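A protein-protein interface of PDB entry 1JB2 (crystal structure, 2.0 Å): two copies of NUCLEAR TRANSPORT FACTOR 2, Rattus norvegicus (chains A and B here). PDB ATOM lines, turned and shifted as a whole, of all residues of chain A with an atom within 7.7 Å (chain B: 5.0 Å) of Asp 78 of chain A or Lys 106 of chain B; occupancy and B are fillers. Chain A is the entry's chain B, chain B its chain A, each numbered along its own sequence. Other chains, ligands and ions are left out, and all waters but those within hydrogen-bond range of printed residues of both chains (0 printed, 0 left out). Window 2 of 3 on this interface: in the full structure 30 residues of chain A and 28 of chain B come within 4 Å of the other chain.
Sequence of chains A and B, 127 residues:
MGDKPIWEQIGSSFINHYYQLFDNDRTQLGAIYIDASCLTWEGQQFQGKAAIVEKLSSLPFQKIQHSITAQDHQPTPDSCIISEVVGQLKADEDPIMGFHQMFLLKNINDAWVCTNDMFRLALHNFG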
ATOM      1  N   PRO A  75     -16.923  -6.280  -5.183  1.00  0.00           N
ATOM      2  CA  PRO A  75     -16.073  -5.284  -4.526  1.00  0.00           C
ATOM      3  C   PRO A  75     -17.036  -4.436  -3.669  1.00  0.00           C
ATOM      4  O   PRO A  75     -18.234  -4.338  -3.994  1.00  0.00           O
ATOM      5  CB  PRO A  75     -15.482  -4.509  -5.700  1.00  0.00           C
ATOM      6  CG  PRO A  75     -16.608  -4.502  -6.698  1.00  0.00           C
ATOM      7  CD  PRO A  75     -17.244  -5.886  -6.574  1.00  0.00           C
ATOM      8  N   THR A  76     -16.545  -3.841  -2.581  1.00  0.00           N
ATOM      9  CA  THR A  76     -17.402  -3.002  -1.721  1.00  0.00           C
ATOM     10  C   THR A  76     -16.814  -1.587  -1.752  1.00  0.00           C
ATOM     11  O   THR A  76     -15.665  -1.408  -2.116  1.00  0.00           O
ATOM     12  CB  THR A  76     -17.443  -3.501  -0.224  1.00  0.00           C
ATOM     13  OG1 THR A  76     -16.294  -3.014   0.485  1.00  0.00           O
ATOM     14  CG2 THR A  76     -17.438  -5.036  -0.150  1.00  0.00           C
ATOM     15  N   PRO A  77     -17.601  -0.560  -1.377  1.00  0.00           N
ATOM     16  CA  PRO A  77     -17.075   0.812  -1.405  1.00  0.00           C
ATOM     17  C   PRO A  77     -15.906   1.130  -0.477  1.00  0.00           C
ATOM     18  O   PRO A  77     -15.207   2.123  -0.675  1.00  0.00           O
ATOM     19  CB  PRO A  77     -18.314   1.659  -1.099  1.00  0.00           C
ATOM     20  CG  PRO A  77     -19.423   0.827  -1.677  1.00  0.00           C
ATOM     21  CD  PRO A  77     -19.061  -0.546  -1.183  1.00  0.00           C
ATOM     22  N   ASP A  78     -15.682   0.310   0.538  1.00  0.00           N
ATOM     23  CA  ASP A  78     -14.559   0.553   1.435  1.00  0.00           C
ATOM     24  C   ASP A  78     -13.352  -0.281   0.998  1.00  0.00           C
ATOM     25  O   ASP A  78     -12.441  -0.499   1.769  1.00  0.00           O
ATOM     26  CB  ASP A  78     -14.923   0.186   2.873  1.00  0.00           C
ATOM     27  CG  ASP A  78     -15.880   1.163   3.502  1.00  0.00           C
ATOM     28  OD1 ASP A  78     -15.567   2.366   3.510  1.00  0.00           O
ATOM     29  OD2 ASP A  78     -16.939   0.736   4.004  1.00  0.00           O
ATOM     30  N   SER A  79     -13.379  -0.761  -0.239  1.00  0.00           N
ATOM     31  CA  SER A  79     -12.302  -1.586  -0.814  1.00  0.00           C
ATOM     32  C   SER A  79     -12.197  -2.998  -0.263  1.00  0.00           C
ATOM     33  O   SER A  79     -11.133  -3.621  -0.316  1.00  0.00           O
ATOM     34  CB  SER A  79     -10.941  -0.889  -0.688  1.00  0.00           C
ATOM     35  OG  SER A  79     -10.916   0.289  -1.472  1.00  0.00           O
ATOM     36  N   CYS A  80     -13.296  -3.522   0.259  1.00  0.00           N
ATOM     37  CA  CYS A  80     -13.275  -4.876   0.749  1.00  0.00           C
ATOM     38  C   CYS A  80     -13.813  -5.761  -0.357  1.00  0.00           C
ATOM     39  O   CYS A  80     -14.233  -5.276  -1.406  1.00  0.00           O
ATOM     40  CB  CYS A  80     -14.152  -5.031   1.990  1.00  0.00           C
ATOM     41  SG  CYS A  80     -13.509  -4.145   3.440  1.00  0.00           S
ATOM     42  N   ILE A  81     -13.786  -7.062  -0.115  1.00  0.00           N
ATOM     43  CA  ILE A  81     -14.314  -8.032  -1.068  1.00  0.00           C
ATOM     44  C   ILE A  81     -15.280  -8.906  -0.287  1.00  0.00           C
ATOM     45  O   ILE A  81     -14.944  -9.398   0.803  1.00  0.00           O
ATOM     46  CB  ILE A  81     -13.200  -8.916  -1.673  1.00  0.00           C
ATOM     47  CG1 ILE A  81     -12.234  -8.044  -2.489  1.00  0.00           C
ATOM     48  CG2 ILE A  81     -13.824 -10.002  -2.578  1.00  0.00           C
ATOM     49  CD1 ILE A  81     -10.980  -8.767  -2.935  1.00  0.00           C
ATOM     50  N   LEU A 105     -13.675  -9.717   3.173  1.00  0.00           N
ATOM     51  CA  LEU A 105     -12.215  -9.611   3.157  1.00  0.00           C
ATOM     52  C   LEU A 105     -11.714  -8.166   3.154  1.00  0.00           C
ATOM     53  O   LEU A 105     -12.290  -7.305   2.500  1.00  0.00           O
ATOM     54  CB  LEU A 105     -11.680 -10.296   1.895  1.00  0.00           C
ATOM     55  CG  LEU A 105     -12.186 -11.712   1.634  1.00  0.00           C
ATOM     56  CD1 LEU A 105     -11.540 -12.220   0.314  1.00  0.00           C
ATOM     57  CD2 LEU A 105     -11.841 -12.637   2.829  1.00  0.00           C
ATOM     58  N   LYS A 106     -10.623  -7.922   3.867  1.00  0.00           N
ATOM     59  CA  LYS A 106     -10.038  -6.590   3.916  1.00  0.00           C
ATOM     60  C   LYS A 106      -8.532  -6.693   3.917  1.00  0.00           C
ATOM     61  O   LYS A 106      -7.976  -7.552   4.576  1.00  0.00           O
ATOM     62  CB  LYS A 106     -10.511  -5.843   5.165  1.00  0.00           C
ATOM     63  CG  LYS A 106     -10.034  -4.387   5.251  1.00  0.00           C
ATOM     64  CD  LYS A 106     -11.069  -3.542   5.970  1.00  0.00           C
ATOM     65  CE  LYS A 106     -10.601  -2.103   6.177  1.00  0.00           C
ATOM     66  NZ  LYS A 106      -9.722  -2.052   7.361  1.00  0.00           N
ATOM     67  N   ASN A 107      -7.874  -5.828   3.157  1.00  0.00           N
ATOM     68  CA  ASN A 107      -6.425  -5.829   3.108  1.00  0.00           C
ATOM     69  C   ASN A 107      -5.868  -4.979   4.248  1.00  0.00           C
ATOM     70  O   ASN A 107      -6.044  -3.764   4.273  1.00  0.00           O
ATOM     71  CB  ASN A 107      -5.908  -5.268   1.778  1.00  0.00           C
ATOM     72  CG  ASN A 107      -4.439  -5.555   1.581  1.00  0.00           C
ATOM     73  OD1 ASN A 107      -4.074  -6.546   0.963  1.00  0.00           O
ATOM     74  ND2 ASN A 107      -3.590  -4.712   2.144  1.00  0.00           N
ATOM     75  N   TRP A 112      -4.569 -10.065   2.852  1.00  0.00           N
ATOM     76  CA  TRP A 112      -6.016 -10.108   2.793  1.00  0.00           C
ATOM     77  C   TRP A 112      -6.470 -10.954   3.979  1.00  0.00           C
ATOM     78  O   TRP A 112      -6.066 -12.102   4.131  1.00  0.00           O
ATOM     79  CB  TRP A 112      -6.503 -10.696   1.461  1.00  0.00           C
ATOM     80  CG  TRP A 112      -6.492  -9.672   0.351  1.00  0.00           C
ATOM     81  CD1 TRP A 112      -5.481  -9.440  -0.532  1.00  0.00           C
ATOM     82  CD2 TRP A 112      -7.479  -8.644   0.103  1.00  0.00           C
ATOM     83  NE1 TRP A 112      -5.765  -8.341  -1.301  1.00  0.00           N
ATOM     84  CE2 TRP A 112      -6.981  -7.831  -0.935  1.00  0.00           C
ATOM     85  CE3 TRP A 112      -8.723  -8.333   0.664  1.00  0.00           C
ATOM     86  CZ2 TRP A 112      -7.683  -6.723  -1.429  1.00  0.00           C
ATOM     87  CZ3 TRP A 112      -9.421  -7.233   0.181  1.00  0.00           C
ATOM     88  CH2 TRP A 112      -8.898  -6.437  -0.860  1.00  0.00           C
ATOM     89  N   ASP B  78     -15.380  -1.438   9.392  1.00  0.00           N
ATOM     90  CA  ASP B  78     -15.602  -0.117   8.831  1.00  0.00           C
ATOM     91  C   ASP B  78     -16.996   0.394   9.164  1.00  0.00           C
ATOM     92  O   ASP B  78     -17.499   1.287   8.494  1.00  0.00           O
ATOM     93  CB  ASP B  78     -15.417  -0.139   7.314  1.00  0.00           C
ATOM     94  CG  ASP B  78     -14.018  -0.557   6.905  1.00  0.00           C
ATOM     95  OD1 ASP B  78     -13.058  -0.097   7.549  1.00  0.00           O
ATOM     96  OD2 ASP B  78     -13.872  -1.337   5.936  1.00  0.00           O
ATOM     97  N   CYS B  80     -19.899  -1.257   8.920  1.00  0.00           N
ATOM     98  CA  CYS B  80     -20.986  -1.701   8.054  1.00  0.00           C
ATOM     99  C   CYS B  80     -21.658  -2.842   8.799  1.00  0.00           C
ATOM    100  O   CYS B  80     -21.214  -3.236   9.880  1.00  0.00           O
ATOM    101  CB  CYS B  80     -20.463  -2.217   6.707  1.00  0.00           C
ATOM    102  SG  CYS B  80     -19.652  -0.970   5.695  1.00  0.00           S
ATOM    103  N   LEU B 104     -24.778  -6.322   2.379  1.00  0.00           N
ATOM    104  CA  LEU B 104     -23.744  -5.584   3.084  1.00  0.00           C
ATOM    105  C   LEU B 104     -24.410  -4.228   3.197  1.00  0.00           C
ATOM    106  O   LEU B 104     -24.831  -3.657   2.192  1.00  0.00           O
ATOM    107  CB  LEU B 104     -22.442  -5.460   2.286  1.00  0.00           C
ATOM    108  CG  LEU B 104     -21.346  -4.786   3.130  1.00  0.00           C
ATOM    109  CD1 LEU B 104     -21.159  -5.581   4.415  1.00  0.00           C
ATOM    110  CD2 LEU B 104     -20.020  -4.687   2.364  1.00  0.00           C
ATOM    111  N   LEU B 105     -24.502  -3.712   4.416  1.00  0.00           N
ATOM    112  CA  LEU B 105     -25.151  -2.433   4.663  1.00  0.00           C
ATOM    113  C   LEU B 105     -24.178  -1.383   5.143  1.00  0.00           C
ATOM    114  O   LEU B 105     -23.251  -1.672   5.898  1.00  0.00           O
ATOM    115  CB  LEU B 105     -26.229  -2.586   5.730  1.00  0.00           C
ATOM    116  CG  LEU B 105     -27.205  -3.741   5.569  1.00  0.00           C
ATOM    117  CD1 LEU B 105     -28.170  -3.689   6.741  1.00  0.00           C
ATOM    118  CD2 LEU B 105     -27.946  -3.658   4.196  1.00  0.00           C
ATOM    119  N   LYS B 106     -24.416  -0.148   4.733  1.00  0.00           N
ATOM    120  CA  LYS B 106     -23.558   0.936   5.155  1.00  0.00           C
ATOM    121  C   LYS B 106     -24.407   2.173   5.324  1.00  0.00           C
ATOM    122  O   LYS B 106     -25.349   2.401   4.570  1.00  0.00           O
ATOM    123  CB  LYS B 106     -22.476   1.193   4.109  1.00  0.00           C
ATOM    124  CG  LYS B 106     -21.424   2.228   4.512  1.00  0.00           C
ATOM    125  CD  LYS B 106     -20.518   2.508   3.329  1.00  0.00           C
ATOM    126  CE  LYS B 106     -19.273   3.312   3.696  1.00  0.00           C
ATOM    127  NZ  LYS B 106     -18.591   3.694   2.418  1.00  0.00           N
ATOM    128  N   ASN B 107     -24.096   2.962   6.338  1.00  0.00           N
ATOM    129  CA  ASN B 107     -24.841   4.184   6.531  1.00  0.00           C
ATOM    130  C   ASN B 107     -24.161   5.242   5.644  1.00  0.00           C
ATOM    131  O   ASN B 107     -22.989   5.556   5.832  1.00  0.00           O
ATOM    132  CB  ASN B 107     -24.801   4.609   7.996  1.00  0.00           C
ATOM    133  CG  ASN B 107     -25.692   5.806   8.269  1.00  0.00           C
ATOM    134  OD1 ASN B 107     -26.752   5.682   8.889  1.00  0.00           O
ATOM    135  ND2 ASN B 107     -25.271   6.973   7.792  1.00  0.00           N
ATOM    136  N   ILE B 108     -24.889   5.762   4.659  1.00  0.00           N
ATOM    137  CA  ILE B 108     -24.341   6.780   3.759  1.00  0.00           C
ATOM    138  C   ILE B 108     -25.312   7.942   3.670  1.00  0.00           C
ATOM    139  O   ILE B 108     -26.517   7.734   3.578  1.00  0.00           O
ATOM    140  CB  ILE B 108     -24.080   6.201   2.353  1.00  0.00           C
ATOM    141  CG1 ILE B 108     -22.938   5.179   2.434  1.00  0.00           C
ATOM    142  CG2 ILE B 108     -23.709   7.319   1.369  1.00  0.00           C
ATOM    143  CD1 ILE B 108     -22.609   4.510   1.135  1.00  0.00           C
ATOM    144  N   ALA B 111     -28.239   7.322   5.930  1.00  0.00           N
ATOM    145  CA  ALA B 111     -29.380   6.453   5.706  1.00  0.00           C
ATOM    146  C   ALA B 111     -28.722   5.112   5.499  1.00  0.00           C
ATOM    147  O   ALA B 111     -27.632   5.039   4.928  1.00  0.00           O
ATOM    148  CB  ALA B 111     -30.153   6.857   4.444  1.00  0.00           C
ATOM    149  N   TRP B 112     -29.353   4.049   5.972  1.00  0.00           N
ATOM    150  CA  TRP B 112     -28.764   2.752   5.735  1.00  0.00           C
ATOM    151  C   TRP B 112     -29.128   2.314   4.310  1.00  0.00           C
ATOM    152  O   TRP B 112     -30.291   2.305   3.935  1.00  0.00           O
ATOM    153  CB  TRP B 112     -29.250   1.751   6.778  1.00  0.00           C
ATOM    154  CG  TRP B 112     -28.536   1.928   8.102  1.00  0.00           C
ATOM    155  CD1 TRP B 112     -28.979   2.618   9.203  1.00  0.00           C
ATOM    156  CD2 TRP B 112     -27.217   1.466   8.424  1.00  0.00           C
ATOM    157  NE1 TRP B 112     -28.008   2.613  10.183  1.00  0.00           N
ATOM    158  CE2 TRP B 112     -26.921   1.914   9.732  1.00  0.00           C
ATOM    159  CE3 TRP B 112     -26.255   0.715   7.729  1.00  0.00           C
ATOM    160  CZ2 TRP B 112     -25.697   1.636  10.362  1.00  0.00           C
ATOM    161  CZ3 TRP B 112     -25.038   0.439   8.352  1.00  0.00           C
ATOM    162  CH2 TRP B 112     -24.772   0.900   9.656  1.00  0.00           C
ATOM    163  N   VAL B 113     -28.114   2.000   3.509  1.00  0.00           N
ATOM    164  CA  VAL B 113     -28.324   1.530   2.139  1.00  0.00           C
ATOM    165  C   VAL B 113     -27.571   0.201   1.953  1.00  0.00           C
ATOM    166  O   VAL B 113     -26.700  -0.157   2.752  1.00  0.00           O
ATOM    167  CB  VAL B 113     -27.796   2.547   1.080  1.00  0.00           C
ATOM    168  CG1 VAL B 113     -28.449   3.918   1.283  1.00  0.00           C
ATOM    169  CG2 VAL B 113     -26.279   2.647   1.156  1.00  0.00           C
ATOM    170  N   THR B 115     -24.949  -1.853  -0.152  1.00  0.00           N
ATOM    171  CA  THR B 115     -23.855  -1.681  -1.103  1.00  0.00           C
ATOM    172  C   THR B 115     -23.562  -2.964  -1.883  1.00  0.00           C
ATOM    173  O   THR B 115     -23.093  -2.908  -3.001  1.00  0.00           O
ATOM    174  CB  THR B 115     -22.535  -1.241  -0.417  1.00  0.00           C
ATOM    175  OG1 THR B 115     -22.070  -2.290   0.449  1.00  0.00           O
ATOM    176  CG2 THR B 115     -22.744   0.060   0.376  1.00  0.00           C
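Among the printed residues, merely in contact across the chains: Thr 76 of chain A with Leu 104 of chain B, Pro 77 of chain A with Thr 115 of chain B and Asp 78 of chain A with Asp 78 of chain B.
Of the 11 printed residues of chain B, 5 touch a printed residue of chain A.
Among the printed residues, Asp or Glu carboxylates within 4 Å of a Lys or Arg side-chain nitrogen of the other chain: Asp 78 of chain A with Lys 106 of chain B (3.5 Å) and Lys 106 of chain A with Asp 78 of chain B (3.9 Å).
OD2 of Asp 78 of chain B lies within hydrogen-bond range of SG of Cys 80 of chain A (3.8 Å).
The side-chain carboxylate (OD1) of Asp 78 of chain B lies within salt-bridge range of the side-chain amino group (NZ) of Lys 106 of chain A (3.9 Å).
OD2 of Asp 78 of chain A is in hydrogen-bond range of SG of Cys 80 of chain B, 3.6 Å away.
The side-chain amino group (NZ) of Lys 106 of chain B lies within salt-bridge range of the side-chain carboxylate (OD1) of Asp 78 of chain A.
Asp 78 of chain A touches its own counterpart, Asp 78 of chain B.
Asp 78 of chain A touches Cys 80 of chain B, and with the chains exchanged Cys 80 of chain A touches Asp 78 of chain B.
Asp 78 of chain A touches Lys 106 of chain B, and with the chains exchanged Lys 106 of chain A touches Asp 78 of chain B.
Positions printed for both chains: 78, 80, 105, 106, 107 and 112.
The side-chain sulfur (SG) of Cys 80 of chain B sits close to the backbone carbonyl oxygen (O) of Leu 105 of chain B.
The backbone carbonyl oxygen (O) of Leu 104 of chain B sits at hydrogen-bond distance from the backbone NH (N) of Thr 115 of chain B, at 3.0 Å.
The backbone NH of Val 113 of chain B lies within hydrogen-bond range of the backbone carbonyl oxygen of Lys 106 of chain B (3.0 Å).
The side-chain hydroxyl (OG1) of Thr 76 of chain A sits close to the backbone NH (N) of Asp 78 of chain A (3.4 Å).
The backbone NH (N) of Cys 80 of chain A is in hydrogen-bond range of the side-chain hydroxyl (OG1) of Thr 76 of chain A.
The side-chain sulfur (SG) of Cys 80 of chain A sits close to the backbone carbonyl oxygen (O) of Leu 105 of chain A, at 3.5 Å.
Of chain B, only Asp 78, Cys 80 and Lys 106 come within 4 Å of Asp 78 of chain A.
Of the printed residues of chain B, Cys 80 of chain A touches Asp 78 (3.8 Å).
Printed residues of chain B within 4 Å of Pro 77 of chain A: Thr 115.
Trp 112 of chain B touches none of the printed residues of chain A.
The nearest printed residue of chain B that does not touch Asp 78 of chain A is Leu 104 of chain B (6.4 Å).
The nearest residue of chain A that does not touch Lys 106 of chain B is Pro 77 of chain A (4.1 Å).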
